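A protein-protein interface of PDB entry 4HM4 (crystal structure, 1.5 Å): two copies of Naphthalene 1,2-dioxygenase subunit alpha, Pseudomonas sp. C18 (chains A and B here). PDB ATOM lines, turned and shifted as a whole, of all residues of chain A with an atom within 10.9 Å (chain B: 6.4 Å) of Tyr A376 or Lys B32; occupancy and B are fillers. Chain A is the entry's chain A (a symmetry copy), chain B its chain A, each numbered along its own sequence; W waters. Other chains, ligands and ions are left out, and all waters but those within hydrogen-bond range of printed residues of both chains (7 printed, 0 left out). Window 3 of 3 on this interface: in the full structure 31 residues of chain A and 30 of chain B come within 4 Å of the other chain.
NH2 of Arg A379 lies within hydrogen-bond range of OE1 of Gln B28 (2.9 Å).
The backbone NH (N) of Tyr A376 lies within hydrogen-bond range of the side-chain carboxylate (OD1) of Asp B62.
OD1 of Asp B62 is in hydrogen-bond range of N of Gln A377, 2.8 Å away.
The side-chain amino group (NZ) of Lys B136 is in hydrogen-bond range of the backbone carbonyl oxygen (O) of Gln A377.
O of Leu B31 sits at hydrogen-bond distance from N of Ala B36.
The backbone NH (N) of Leu A19 sits at hydrogen-bond distance from the backbone carbonyl oxygen (O) of Arg A379 (3.0 Å).
The backbone carbonyl oxygen (O) of Gly A22 is in hydrogen-bond range of the side-chain amino group (NZ) of Lys A374 (2.7 Å).
The side-chain amide oxygen (OD1) of Asn A372 lies within hydrogen-bond range of the side-chain amino group (NZ) of Lys A375.
O of Lys A374 sits at hydrogen-bond distance from NE of Arg A379 (2.8 Å).
O of Gln A377 sits at hydrogen-bond distance from OG of Ser A381.
Lys A375 touches Ile B61.
CB of Lys A375 touches OD1 of Asp B62, 3.5 Å away.
CD1 of Tyr A376 touches CB of Leu B31, 3.9 Å away.
Lys B32 touches Tyr A376.
Ala B36 touches Tyr A376.
Ile B61 touches Tyr A376 (CD1 to N, 3.8 Å).
Ala B36 touches Gln A377 (CB to NE2, 3.8 Å).
CG of Phe B152 touches NE2 of Gln A377, at 3.6 Å.
NH2 of Arg A379 touches CD1 of Leu B31, at 3.7 Å.
Arg A379 touches Ile B61.
Of chain B, only Leu B31 (3.9 Å), Lys B32 (3.3 Å), Ala B36 (3.7 Å), Ile B61 (3.8 Å) and Asp B62 (3.4 Å) come within 4 Å of Tyr A376.
Of chain A, only Tyr A376 (3.3 Å) comes within 4 Å of Lys B32.
His B29 touches none of the printed residues of chain A.
Leu B31 touches just these residues of chain A: Tyr A376 (3.9 Å) and Arg A379 (3.7 Å).
Of the printed residues of chain B, Gln A377 touches Ala B36 (3.8 Å), Asp B62 (2.8 Å), Lys B136 (2.8 Å) and Phe B152 (3.6 Å).
Of the printed residues of chain A, Gln B28 touches Arg A379.
Printed residues of chain A within 4 Å of Asp B62: Lys A375, Tyr A376 and Gln A377.
The nearest residue of chain A that does not touch Lys B32 is Arg A379 (7.0 Å).
The nearest printed residue of chain B that does not touch Arg A379 is Asp B62 (6.4 Å).
Printed residues of chain B that touch a printed residue of chain A: Gln B28, Leu B31, Lys B32, Ala B36, Ile B61, Asp B62, Lys B136 and Phe B152.
Hydrophobic or aromatic side chains of chain B within 4 Å of the printed part of chain A: Leu B31, Ala B36, Ile B61 and Phe B152.
Among the printed residues, 15 pairs touch across the chains.
No position is printed for both chains.
Of the 15 pairs that touch across the chains among the printed residues, none has its exchanged pair printed and touching as well.
Water W2 bridges the backbone carbonyl oxygen (O) of Gln B28 and the guanidinium group (NH1) of Arg A379.
Water W5 bridges the side-chain amino group (NZ) of Lys B136 (3.0 Å) and the side-chain amide oxygen (OE1) of Gln A377 (3.3 Å).
Water W6 lies within hydrogen-bond range of the side-chain amide nitrogen of Gln B28 (3.0 Å) and the guanidinium group of Arg A379 (3.1 Å).
Water W3 lies within hydrogen-bond range of the side-chain amino group (NZ) of Lys B136 (3.2 Å) and the side-chain hydroxyl (OG) of Ser A381 (3.3 Å).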
ATOM      1  N   LYS A  17      -5.851   3.046  30.851  1.00  0.00           N
ATOM      2  CA  LYS A  17      -6.427   4.373  30.635  1.00  0.00           C
ATOM      3  C   LYS A  17      -7.909   4.356  30.993  1.00  0.00           C
ATOM      4  O   LYS A  17      -8.644   3.450  30.598  1.00  0.00           O
ATOM      5  CB  LYS A  17      -6.224   4.849  29.188  1.00  0.00           C
ATOM      6  CG  LYS A  17      -4.770   5.169  28.836  1.00  0.00           C
ATOM      7  CD  LYS A  17      -4.231   6.284  29.735  1.00  0.00           C
ATOM      8  CE  LYS A  17      -2.810   6.696  29.371  1.00  0.00           C
ATOM      9  NZ  LYS A  17      -2.270   7.737  30.307  1.00  0.00           N
ATOM     10  N   HIS A  18      -8.347   5.355  31.755  1.00  0.00           N
ATOM     11  CA  HIS A  18      -9.713   5.384  32.265  1.00  0.00           C
ATOM     12  C   HIS A  18     -10.722   5.404  31.116  1.00  0.00           C
ATOM     13  O   HIS A  18     -11.844   4.908  31.263  1.00  0.00           O
ATOM     14  CB  HIS A  18      -9.883   6.594  33.191  1.00  0.00           C
ATOM     15  CG  HIS A  18     -11.018   6.479  34.165  1.00  0.00           C
ATOM     16  ND1 HIS A  18     -11.109   7.276  35.286  1.00  0.00           N
ATOM     17  CD2 HIS A  18     -12.111   5.680  34.184  1.00  0.00           C
ATOM     18  CE1 HIS A  18     -12.202   6.969  35.957  1.00  0.00           C
ATOM     19  NE2 HIS A  18     -12.833   6.004  35.308  1.00  0.00           N
ATOM     20  N   LEU A  19     -10.318   5.944  29.965  1.00  0.00           N
ATOM     21  CA  LEU A  19     -11.201   5.977  28.796  1.00  0.00           C
ATOM     22  C   LEU A  19     -11.721   4.600  28.375  1.00  0.00           C
ATOM     23  O   LEU A  19     -12.756   4.509  27.715  1.00  0.00           O
ATOM     24  CB  LEU A  19     -10.523   6.657  27.599  1.00  0.00           C
ATOM     25  CG  LEU A  19      -9.387   5.892  26.905  1.00  0.00           C
ATOM     26  CD1 LEU A  19      -9.883   5.008  25.756  1.00  0.00           C
ATOM     27  CD2 LEU A  19      -8.327   6.857  26.403  1.00  0.00           C
ATOM     28  N   GLY A  22     -15.317   4.193  29.065  1.00  0.00           N
ATOM     29  CA  GLY A  22     -16.288   5.149  28.550  1.00  0.00           C
ATOM     30  C   GLY A  22     -16.288   5.407  27.051  1.00  0.00           C
ATOM     31  O   GLY A  22     -17.228   6.001  26.525  1.00  0.00           O
ATOM     32  N   ASP A  23     -15.260   4.952  26.346  1.00  0.00           N
ATOM     33  CA  ASP A  23     -15.082   5.373  24.956  1.00  0.00           C
ATOM     34  C   ASP A  23     -15.925   4.502  24.024  1.00  0.00           C
ATOM     35  O   ASP A  23     -15.713   3.287  23.951  1.00  0.00           O
ATOM     36  CB  ASP A  23     -13.592   5.289  24.584  1.00  0.00           C
ATOM     37  CG  ASP A  23     -13.282   5.897  23.235  1.00  0.00           C
ATOM     38  OD1 ASP A  23     -13.683   5.319  22.204  1.00  0.00           O
ATOM     39  OD2 ASP A  23     -12.605   6.946  23.197  1.00  0.00           O
ATOM     40  N   ASN A 322     -21.319   2.589  28.569  1.00  0.00           N
ATOM     41  CA  ASN A 322     -21.796   2.794  29.938  1.00  0.00           C
ATOM     42  C   ASN A 322     -23.123   2.079  30.205  1.00  0.00           C
ATOM     43  O   ASN A 322     -23.918   2.549  31.012  1.00  0.00           O
ATOM     44  CB  ASN A 322     -21.962   4.292  30.277  1.00  0.00           C
ATOM     45  CG  ASN A 322     -20.647   5.001  30.647  1.00  0.00           C
ATOM     46  OD1 ASN A 322     -20.658   6.211  30.911  1.00  0.00           O
ATOM     47  ND2 ASN A 322     -19.526   4.279  30.648  1.00  0.00           N
ATOM     48  N   SER A 370     -17.239   3.758  35.708  1.00  0.00           N
ATOM     49  CA  SER A 370     -17.443   3.675  34.266  1.00  0.00           C
ATOM     50  C   SER A 370     -17.734   5.040  33.660  1.00  0.00           C
ATOM     51  O   SER A 370     -17.134   5.422  32.653  1.00  0.00           O
ATOM     52  CB  SER A 370     -18.571   2.704  33.912  1.00  0.00           C
ATOM     53  OG  SER A 370     -18.283   1.404  34.388  1.00  0.00           O
ATOM     54  N   GLN A 371     -18.661   5.775  34.263  1.00  0.00           N
ATOM     55  CA  GLN A 371     -19.089   7.048  33.700  1.00  0.00           C
ATOM     56  C   GLN A 371     -17.974   8.101  33.749  1.00  0.00           C
ATOM     57  O   GLN A 371     -17.867   8.959  32.860  1.00  0.00           O
ATOM     58  CB  GLN A 371     -20.363   7.517  34.406  1.00  0.00           C
ATOM     59  CG  GLN A 371     -21.530   6.572  34.143  1.00  0.00           C
ATOM     60  CD  GLN A 371     -22.737   6.858  35.001  1.00  0.00           C
ATOM     61  OE1 GLN A 371     -22.934   7.982  35.455  1.00  0.00           O
ATOM     62  NE2 GLN A 371     -23.554   5.835  35.240  1.00  0.00           N
ATOM     63  N   ASN A 372     -17.123   8.019  34.763  1.00  0.00           N
ATOM     64  CA  ASN A 372     -15.998   8.938  34.854  1.00  0.00           C
ATOM     65  C   ASN A 372     -15.019   8.771  33.695  1.00  0.00           C
ATOM     66  O   ASN A 372     -14.265   9.689  33.386  1.00  0.00           O
ATOM     67  CB  ASN A 372     -15.277   8.789  36.204  1.00  0.00           C
ATOM     68  CG  ASN A 372     -16.064   9.400  37.339  1.00  0.00           C
ATOM     69  OD1 ASN A 372     -16.888  10.283  37.113  1.00  0.00           O
ATOM     70  ND2 ASN A 372     -15.821   8.940  38.561  1.00  0.00           N
ATOM     71  N   GLY A 373     -15.043   7.604  33.053  1.00  0.00           N
ATOM     72  CA  GLY A 373     -14.187   7.349  31.905  1.00  0.00           C
ATOM     73  C   GLY A 373     -14.539   8.180  30.680  1.00  0.00           C
ATOM     74  O   GLY A 373     -13.752   8.254  29.734  1.00  0.00           O
ATOM     75  N   LYS A 374     -15.721   8.794  30.691  1.00  0.00           N
ATOM     76  CA  LYS A 374     -16.134   9.702  29.620  1.00  0.00           C
ATOM     77  C   LYS A 374     -15.724  11.145  29.908  1.00  0.00           C
ATOM     78  O   LYS A 374     -15.642  11.966  28.990  1.00  0.00           O
ATOM     79  CB  LYS A 374     -17.650   9.667  29.421  1.00  0.00           C
ATOM     80  CG  LYS A 374     -18.180   8.372  28.817  1.00  0.00           C
ATOM     81  CD  LYS A 374     -19.686   8.463  28.562  1.00  0.00           C
ATOM     82  CE  LYS A 374     -20.228   7.252  27.792  1.00  0.00           C
ATOM     83  NZ  LYS A 374     -19.680   7.151  26.407  1.00  0.00           N
ATOM     84  N   LYS A 375     -15.476  11.453  31.179  1.00  0.00           N
ATOM     85  CA  LYS A 375     -15.201  12.832  31.581  1.00  0.00           C
ATOM     86  C   LYS A 375     -13.855  13.311  31.062  1.00  0.00           C
ATOM     87  O   LYS A 375     -12.855  12.586  31.133  1.00  0.00           O
ATOM     88  CB  LYS A 375     -15.309  13.002  33.103  1.00  0.00           C
ATOM     89  CG  LYS A 375     -16.736  12.825  33.626  1.00  0.00           C
ATOM     90  CD  LYS A 375     -16.848  13.187  35.101  1.00  0.00           C
ATOM     91  CE  LYS A 375     -18.298  13.211  35.563  1.00  0.00           C
ATOM     92  NZ  LYS A 375     -18.893  11.842  35.609  1.00  0.00           N
ATOM     93  N   TYR A 376     -13.849  14.530  30.529  1.00  0.00           N
ATOM     94  CA  TYR A 376     -12.693  15.055  29.808  1.00  0.00           C
ATOM     95  C   TYR A 376     -11.358  14.937  30.554  1.00  0.00           C
ATOM     96  O   TYR A 376     -10.348  14.518  29.972  1.00  0.00           O
ATOM     97  CB  TYR A 376     -12.932  16.510  29.365  1.00  0.00           C
ATOM     98  CG  TYR A 376     -11.784  17.076  28.553  1.00  0.00           C
ATOM     99  CD1 TYR A 376     -11.712  16.873  27.174  1.00  0.00           C
ATOM    100  CD2 TYR A 376     -10.764  17.795  29.163  1.00  0.00           C
ATOM    101  CE1 TYR A 376     -10.658  17.387  26.422  1.00  0.00           C
ATOM    102  CE2 TYR A 376      -9.703  18.303  28.424  1.00  0.00           C
ATOM    103  CZ  TYR A 376      -9.652  18.096  27.056  1.00  0.00           C
ATOM    104  OH  TYR A 376      -8.593  18.603  26.327  1.00  0.00           O
ATOM    105  N   GLN A 377     -11.337  15.329  31.826  1.00  0.00           N
ATOM    106  CA  GLN A 377     -10.079  15.357  32.572  1.00  0.00           C
ATOM    107  C   GLN A 377      -9.654  13.974  33.047  1.00  0.00           C
ATOM    108  O   GLN A 377      -8.544  13.804  33.566  1.00  0.00           O
ATOM    109  CB  GLN A 377     -10.158  16.326  33.756  1.00  0.00           C
ATOM    110  CG  GLN A 377     -10.288  17.795  33.351  1.00  0.00           C
ATOM    111  CD  GLN A 377      -9.017  18.355  32.736  1.00  0.00           C
ATOM    112  OE1 GLN A 377      -7.907  17.879  33.005  1.00  0.00           O
ATOM    113  NE2 GLN A 377      -9.175  19.369  31.892  1.00  0.00           N
ATOM    114  N   SER A 378     -10.522  12.981  32.860  1.00  0.00           N
ATOM    115  CA  SER A 378     -10.223  11.625  33.335  1.00  0.00           C
ATOM    116  C   SER A 378      -9.897  10.626  32.233  1.00  0.00           C
ATOM    117  O   SER A 378      -9.364   9.559  32.520  1.00  0.00           O
ATOM    118  CB  SER A 378     -11.364  11.070  34.196  1.00  0.00           C
ATOM    119  OG  SER A 378     -11.460  11.753  35.426  1.00  0.00           O
ATOM    120  N   ARG A 379     -10.233  10.950  30.985  1.00  0.00           N
ATOM    121  CA  ARG A 379     -10.049  10.008  29.881  1.00  0.00           C
ATOM    122  C   ARG A 379      -8.627   9.465  29.805  1.00  0.00           C
ATOM    123  O   ARG A 379      -8.429   8.259  29.619  1.00  0.00           O
ATOM    124  CB  ARG A 379     -10.422  10.656  28.542  1.00  0.00           C
ATOM    125  CG  ARG A 379     -11.902  10.977  28.380  1.00  0.00           C
ATOM    126  CD  ARG A 379     -12.147  11.912  27.197  1.00  0.00           C
ATOM    127  NE  ARG A 379     -13.511  12.435  27.206  1.00  0.00           N
ATOM    128  CZ  ARG A 379     -13.979  13.357  26.365  1.00  0.00           C
ATOM    129  NH1 ARG A 379     -13.199  13.883  25.421  1.00  0.00           N
ATOM    130  NH2 ARG A 379     -15.233  13.764  26.477  1.00  0.00           N
ATOM    131  N   ASP A 380      -7.644  10.352  29.960  1.00  0.00           N
ATOM    132  CA  ASP A 380      -6.227   9.992  29.833  1.00  0.00           C
ATOM    133  C   ASP A 380      -5.581   9.674  31.186  1.00  0.00           C
ATOM    134  O   ASP A 380      -4.351   9.549  31.297  1.00  0.00           O
ATOM    135  CB  ASP A 380      -5.475  11.138  29.124  1.00  0.00           C
ATOM    136  CG  ASP A 380      -4.010  10.815  28.831  1.00  0.00           C
ATOM    137  OD1 ASP A 380      -3.725   9.741  28.247  1.00  0.00           O
ATOM    138  OD2 ASP A 380      -3.139  11.648  29.187  1.00  0.00           O
ATOM    139  N   SER A 381      -6.403   9.524  32.217  1.00  0.00           N
ATOM    140  CA  SER A 381      -5.881   9.186  33.536  1.00  0.00           C
ATOM    141  C   SER A 381      -5.658   7.683  33.671  1.00  0.00           C
ATOM    142  O   SER A 381      -6.208   6.898  32.901  1.00  0.00           O
ATOM    143  CB  SER A 381      -6.811   9.691  34.628  1.00  0.00           C
ATOM    144  OG  SER A 381      -6.893  11.105  34.575  1.00  0.00           O
ATOM    145  N   ASP A 382      -4.858   7.295  34.660  1.00  0.00           N
ATOM    146  CA  ASP A 382      -4.446   5.906  34.815  1.00  0.00           C
ATOM    147  C   ASP A 382      -5.140   5.217  35.987  1.00  0.00           C
ATOM    148  O   ASP A 382      -4.969   5.619  37.145  1.00  0.00           O
ATOM    149  CB  ASP A 382      -2.925   5.837  34.995  1.00  0.00           C
ATOM    150  CG  ASP A 382      -2.183   6.509  33.864  1.00  0.00           C
ATOM    151  OD1 ASP A 382      -2.415   6.122  32.701  1.00  0.00           O
ATOM    152  OD2 ASP A 382      -1.388   7.436  34.127  1.00  0.00           O
ATOM    153  N   PHE B  27     -18.982  20.383  20.211  1.00  0.00           N
ATOM    154  CA  PHE B  27     -19.137  20.341  21.658  1.00  0.00           C
ATOM    155  C   PHE B  27     -17.927  19.647  22.296  1.00  0.00           C
ATOM    156  O   PHE B  27     -17.362  20.133  23.271  1.00  0.00           O
ATOM    157  CB  PHE B  27     -20.440  19.628  22.059  1.00  0.00           C
ATOM    158  CG  PHE B  27     -20.631  19.520  23.547  1.00  0.00           C
ATOM    159  CD1 PHE B  27     -20.077  18.460  24.261  1.00  0.00           C
ATOM    160  CD2 PHE B  27     -21.359  20.481  24.237  1.00  0.00           C
ATOM    161  CE1 PHE B  27     -20.245  18.360  25.645  1.00  0.00           C
ATOM    162  CE2 PHE B  27     -21.530  20.390  25.612  1.00  0.00           C
ATOM    163  CZ  PHE B  27     -20.977  19.331  26.317  1.00  0.00           C
ATOM    164  N   GLN B  28     -17.534  18.504  21.751  1.00  0.00           N
ATOM    165  CA  GLN B  28     -16.357  17.802  22.258  1.00  0.00           C
ATOM    166  C   GLN B  28     -15.091  18.661  22.119  1.00  0.00           C
ATOM    167  O   GLN B  28     -14.248  18.693  23.021  1.00  0.00           O
ATOM    168  CB  GLN B  28     -16.195  16.449  21.564  1.00  0.00           C
ATOM    169  CG  GLN B  28     -17.311  15.453  21.909  1.00  0.00           C
ATOM    170  CD  GLN B  28     -17.277  15.043  23.373  1.00  0.00           C
ATOM    171  OE1 GLN B  28     -16.207  14.718  23.906  1.00  0.00           O
ATOM    172  NE2 GLN B  28     -18.439  15.069  24.039  1.00  0.00           N
ATOM    173  N   HIS B  29     -14.973  19.377  21.005  1.00  0.00           N
ATOM    174  CA  HIS B  29     -13.865  20.311  20.808  1.00  0.00           C
ATOM    175  C   HIS B  29     -13.889  21.471  21.817  1.00  0.00           C
ATOM    176  O   HIS B  29     -12.834  21.940  22.259  1.00  0.00           O
ATOM    177  CB  HIS B  29     -13.882  20.845  19.373  1.00  0.00           C
ATOM    178  CG  HIS B  29     -12.722  21.731  19.038  1.00  0.00           C
ATOM    179  ND1 HIS B  29     -11.434  21.258  18.905  1.00  0.00           N
ATOM    180  CD2 HIS B  29     -12.660  23.063  18.790  1.00  0.00           C
ATOM    181  CE1 HIS B  29     -10.628  22.260  18.598  1.00  0.00           C
ATOM    182  NE2 HIS B  29     -11.348  23.368  18.528  1.00  0.00           N
ATOM    183  N   GLU B  30     -15.082  21.943  22.169  1.00  0.00           N
ATOM    184  CA  GLU B  30     -15.227  22.990  23.182  1.00  0.00           C
ATOM    185  C   GLU B  30     -14.753  22.524  24.557  1.00  0.00           C
ATOM    186  O   GLU B  30     -14.281  23.328  25.359  1.00  0.00           O
ATOM    187  CB  GLU B  30     -16.682  23.455  23.292  1.00  0.00           C
ATOM    188  CG  GLU B  30     -17.224  24.238  22.117  1.00  0.00           C
ATOM    189  CD  GLU B  30     -18.707  24.526  22.268  1.00  0.00           C
ATOM    190  OE1 GLU B  30     -19.346  23.881  23.131  1.00  0.00           O
ATOM    191  OE2 GLU B  30     -19.236  25.392  21.544  1.00  0.00           O
ATOM    192  N   LEU B  31     -14.899  21.238  24.854  1.00  0.00           N
ATOM    193  CA  LEU B  31     -14.416  20.739  26.143  1.00  0.00           C
ATOM    194  C   LEU B  31     -12.926  21.048  26.269  1.00  0.00           C
ATOM    195  O   LEU B  31     -12.452  21.480  27.325  1.00  0.00           O
ATOM    196  CB  LEU B  31     -14.680  19.241  26.301  1.00  0.00           C
ATOM    197  CG  LEU B  31     -16.140  18.808  26.259  1.00  0.00           C
ATOM    198  CD1 LEU B  31     -16.248  17.294  26.418  1.00  0.00           C
ATOM    199  CD2 LEU B  31     -16.921  19.525  27.346  1.00  0.00           C
ATOM    200  N   LYS B  32     -12.197  20.857  25.173  1.00  0.00           N
ATOM    201  CA  LYS B  32     -10.769  21.167  25.139  1.00  0.00           C
ATOM    202  C   LYS B  32     -10.452  22.664  25.069  1.00  0.00           C
ATOM    203  O   LYS B  32      -9.696  23.185  25.892  1.00  0.00           O
ATOM    204  CB  LYS B  32     -10.100  20.439  23.968  1.00  0.00           C
ATOM    205  CG  LYS B  32      -8.624  20.779  23.801  1.00  0.00           C
ATOM    206  CD  LYS B  32      -7.959  19.865  22.786  1.00  0.00           C
ATOM    207  CE  LYS B  32      -8.514  20.066  21.393  1.00  0.00           C
ATOM    208  NZ  LYS B  32      -7.787  19.209  20.401  1.00  0.00           N
ATOM    209  N   THR B  33     -11.029  23.354  24.090  1.00  0.00           N
ATOM    210  CA  THR B  33     -10.615  24.730  23.772  1.00  0.00           C
ATOM    211  C   THR B  33     -11.372  25.834  24.509  1.00  0.00           C
ATOM    212  O   THR B  33     -10.920  26.989  24.528  1.00  0.00           O
ATOM    213  CB  THR B  33     -10.706  25.001  22.263  1.00  0.00           C
ATOM    214  OG1 THR B  33     -12.058  24.822  21.833  1.00  0.00           O
ATOM    215  CG2 THR B  33      -9.795  24.057  21.487  1.00  0.00           C
ATOM    216  N   ILE B  34     -12.523  25.496  25.089  1.00  0.00           N
ATOM    217  CA  ILE B  34     -13.287  26.456  25.888  1.00  0.00           C
ATOM    218  C   ILE B  34     -13.218  26.106  27.372  1.00  0.00           C
ATOM    219  O   ILE B  34     -12.706  26.886  28.173  1.00  0.00           O
ATOM    220  CB  ILE B  34     -14.775  26.556  25.450  1.00  0.00           C
ATOM    221  CG1 ILE B  34     -14.902  27.017  23.989  1.00  0.00           C
ATOM    222  CG2 ILE B  34     -15.546  27.486  26.385  1.00  0.00           C
ATOM    223  CD1 ILE B  34     -14.360  28.415  23.716  1.00  0.00           C
ATOM    224  N   PHE B  35     -13.712  24.924  27.738  1.00  0.00           N
ATOM    225  CA  PHE B  35     -13.868  24.589  29.151  1.00  0.00           C
ATOM    226  C   PHE B  35     -12.582  24.196  29.889  1.00  0.00           C
ATOM    227  O   PHE B  35     -12.421  24.530  31.062  1.00  0.00           O
ATOM    228  CB  PHE B  35     -14.994  23.567  29.337  1.00  0.00           C
ATOM    229  CG  PHE B  35     -16.334  24.102  28.923  1.00  0.00           C
ATOM    230  CD1 PHE B  35     -17.023  24.989  29.749  1.00  0.00           C
ATOM    231  CD2 PHE B  35     -16.877  23.780  27.686  1.00  0.00           C
ATOM    232  CE1 PHE B  35     -18.246  25.508  29.364  1.00  0.00           C
ATOM    233  CE2 PHE B  35     -18.104  24.290  27.295  1.00  0.00           C
ATOM    234  CZ  PHE B  35     -18.786  25.163  28.131  1.00  0.00           C
ATOM    235  N   ALA B  36     -11.649  23.533  29.208  1.00  0.00           N
ATOM    236  CA  ALA B  36     -10.383  23.169  29.849  1.00  0.00           C
ATOM    237  C   ALA B  36      -9.389  24.331  29.852  1.00  0.00           C
ATOM    238  O   ALA B  36      -8.339  24.256  30.495  1.00  0.00           O
ATOM    239  CB  ALA B  36      -9.767  21.937  29.183  1.00  0.00           C
ATOM    240  N   ARG B  37      -9.737  25.409  29.151  1.00  0.00           N
ATOM    241  CA  ARG B  37      -8.821  26.529  28.940  1.00  0.00           C
ATOM    242  C   ARG B  37      -9.174  27.792  29.729  1.00  0.00           C
ATOM    243  O   ARG B  37      -8.294  28.581  30.093  1.00  0.00           O
ATOM    244  CB  ARG B  37      -8.762  26.885  27.453  1.00  0.00           C
ATOM    245  CG  ARG B  37      -7.742  27.990  27.163  1.00  0.00           C
ATOM    246  CD  ARG B  37      -7.551  28.258  25.712  1.00  0.00           C
ATOM    247  NE  ARG B  37      -7.194  27.057  24.976  1.00  0.00           N
ATOM    248  CZ  ARG B  37      -7.408  26.916  23.677  1.00  0.00           C
ATOM    249  NH1 ARG B  37      -7.976  27.912  22.999  1.00  0.00           N
ATOM    250  NH2 ARG B  37      -7.060  25.796  23.063  1.00  0.00           N
ATOM    251  N   ASN B  38     -10.464  27.990  29.978  1.00  0.00           N
ATOM    252  CA  ASN B  38     -10.955  29.253  30.530  1.00  0.00           C
ATOM    253  C   ASN B  38     -11.372  29.190  32.000  1.00  0.00           C
ATOM    254  O   ASN B  38     -11.388  28.117  32.604  1.00  0.00           O
ATOM    255  CB  ASN B  38     -12.103  29.786  29.664  1.00  0.00           C
ATOM    256  CG  ASN B  38     -11.626  30.273  28.310  1.00  0.00           C
ATOM    257  OD1 ASN B  38     -11.109  31.380  28.198  1.00  0.00           O
ATOM    258  ND2 ASN B  38     -11.783  29.443  27.279  1.00  0.00           N
ATOM    259  N   ILE B  61     -17.783  19.252  31.734  1.00  0.00           N
ATOM    260  CA  ILE B  61     -18.462  18.012  32.112  1.00  0.00           C
ATOM    261  C   ILE B  61     -17.761  17.308  33.277  1.00  0.00           C
ATOM    262  O   ILE B  61     -18.245  16.287  33.789  1.00  0.00           O
ATOM    263  CB  ILE B  61     -18.618  17.042  30.911  1.00  0.00           C
ATOM    264  CG1 ILE B  61     -17.256  16.564  30.394  1.00  0.00           C
ATOM    265  CG2 ILE B  61     -19.439  17.696  29.801  1.00  0.00           C
ATOM    266  CD1 ILE B  61     -17.351  15.394  29.395  1.00  0.00           C
ATOM    267  N   ASP B  62     -16.623  17.849  33.708  1.00  0.00           N
ATOM    268  CA  ASP B  62     -15.919  17.273  34.853  1.00  0.00           C
ATOM    269  C   ASP B  62     -16.535  17.744  36.159  1.00  0.00           C
ATOM    270  O   ASP B  62     -17.118  18.833  36.213  1.00  0.00           O
ATOM    271  CB  ASP B  62     -14.444  17.663  34.808  1.00  0.00           C
ATOM    272  CG  ASP B  62     -13.746  17.089  33.605  1.00  0.00           C
ATOM    273  OD1 ASP B  62     -13.407  15.889  33.636  1.00  0.00           O
ATOM    274  OD2 ASP B  62     -13.553  17.828  32.618  1.00  0.00           O
ATOM    275  N   LYS B 136      -6.247  14.656  41.357  1.00  0.00           N
ATOM    276  CA  LYS B 136      -5.862  15.535  40.253  1.00  0.00           C
ATOM    277  C   LYS B 136      -6.348  16.952  40.545  1.00  0.00           C
ATOM    278  O   LYS B 136      -7.550  17.201  40.645  1.00  0.00           O
ATOM    279  CB  LYS B 136      -6.423  15.016  38.925  1.00  0.00           C
ATOM    280  CG  LYS B 136      -6.065  15.875  37.716  1.00  0.00           C
ATOM    281  CD  LYS B 136      -6.303  15.109  36.413  1.00  0.00           C
ATOM    282  CE  LYS B 136      -6.042  15.984  35.199  1.00  0.00           C
ATOM    283  NZ  LYS B 136      -6.097  15.214  33.931  1.00  0.00           N
ATOM    284  N   PHE B 152      -8.357  24.872  34.578  1.00  0.00           N
ATOM    285  CA  PHE B 152      -7.462  23.718  34.421  1.00  0.00           C
ATOM    286  C   PHE B 152      -6.137  24.058  33.726  1.00  0.00           C
ATOM    287  O   PHE B 152      -5.169  23.293  33.804  1.00  0.00           O
ATOM    288  CB  PHE B 152      -8.166  22.592  33.643  1.00  0.00           C
ATOM    289  CG  PHE B 152      -9.222  21.852  34.434  1.00  0.00           C
ATOM    290  CD1 PHE B 152      -8.874  21.097  35.548  1.00  0.00           C
ATOM    291  CD2 PHE B 152     -10.554  21.862  34.023  1.00  0.00           C
ATOM    292  CE1 PHE B 152      -9.837  20.393  36.267  1.00  0.00           C
ATOM    293  CE2 PHE B 152     -11.527  21.161  34.735  1.00  0.00           C
ATOM    294  CZ  PHE B 152     -11.166  20.422  35.858  1.00  0.00           C
ATOM    295  N   SER B 427      -4.751  26.460  19.766  1.00  0.00           N
ATOM    296  CA  SER B 427      -4.327  25.274  20.513  1.00  0.00           C
ATOM    297  C   SER B 427      -3.896  25.579  21.944  1.00  0.00           C
ATOM    298  O   SER B 427      -3.689  24.662  22.737  1.00  0.00           O
ATOM    299  CB  SER B 427      -3.177  24.562  19.792  1.00  0.00           C
ATOM    300  OG  SER B 427      -3.529  24.206  18.471  1.00  0.00           O
HETATM  301  O   HOH W   1      -6.073  12.724  32.282  1.00  0.00           O
HETATM  302  O   HOH W   2     -13.080  16.251  23.799  1.00  0.00           O
HETATM  303  O   HOH W   3      -4.056  12.867  34.792  1.00  0.00           O
HETATM  304  O   HOH W   4     -13.088  13.918  35.590  1.00  0.00           O
HETATM  305  O   HOH W   5      -5.497  16.400  31.265  1.00  0.00           O
HETATM  306  O   HOH W   6     -18.358  13.604  26.648  1.00  0.00           O
HETATM  307  O   HOH W   7     -14.453  13.276  22.368  1.00  0.00           O
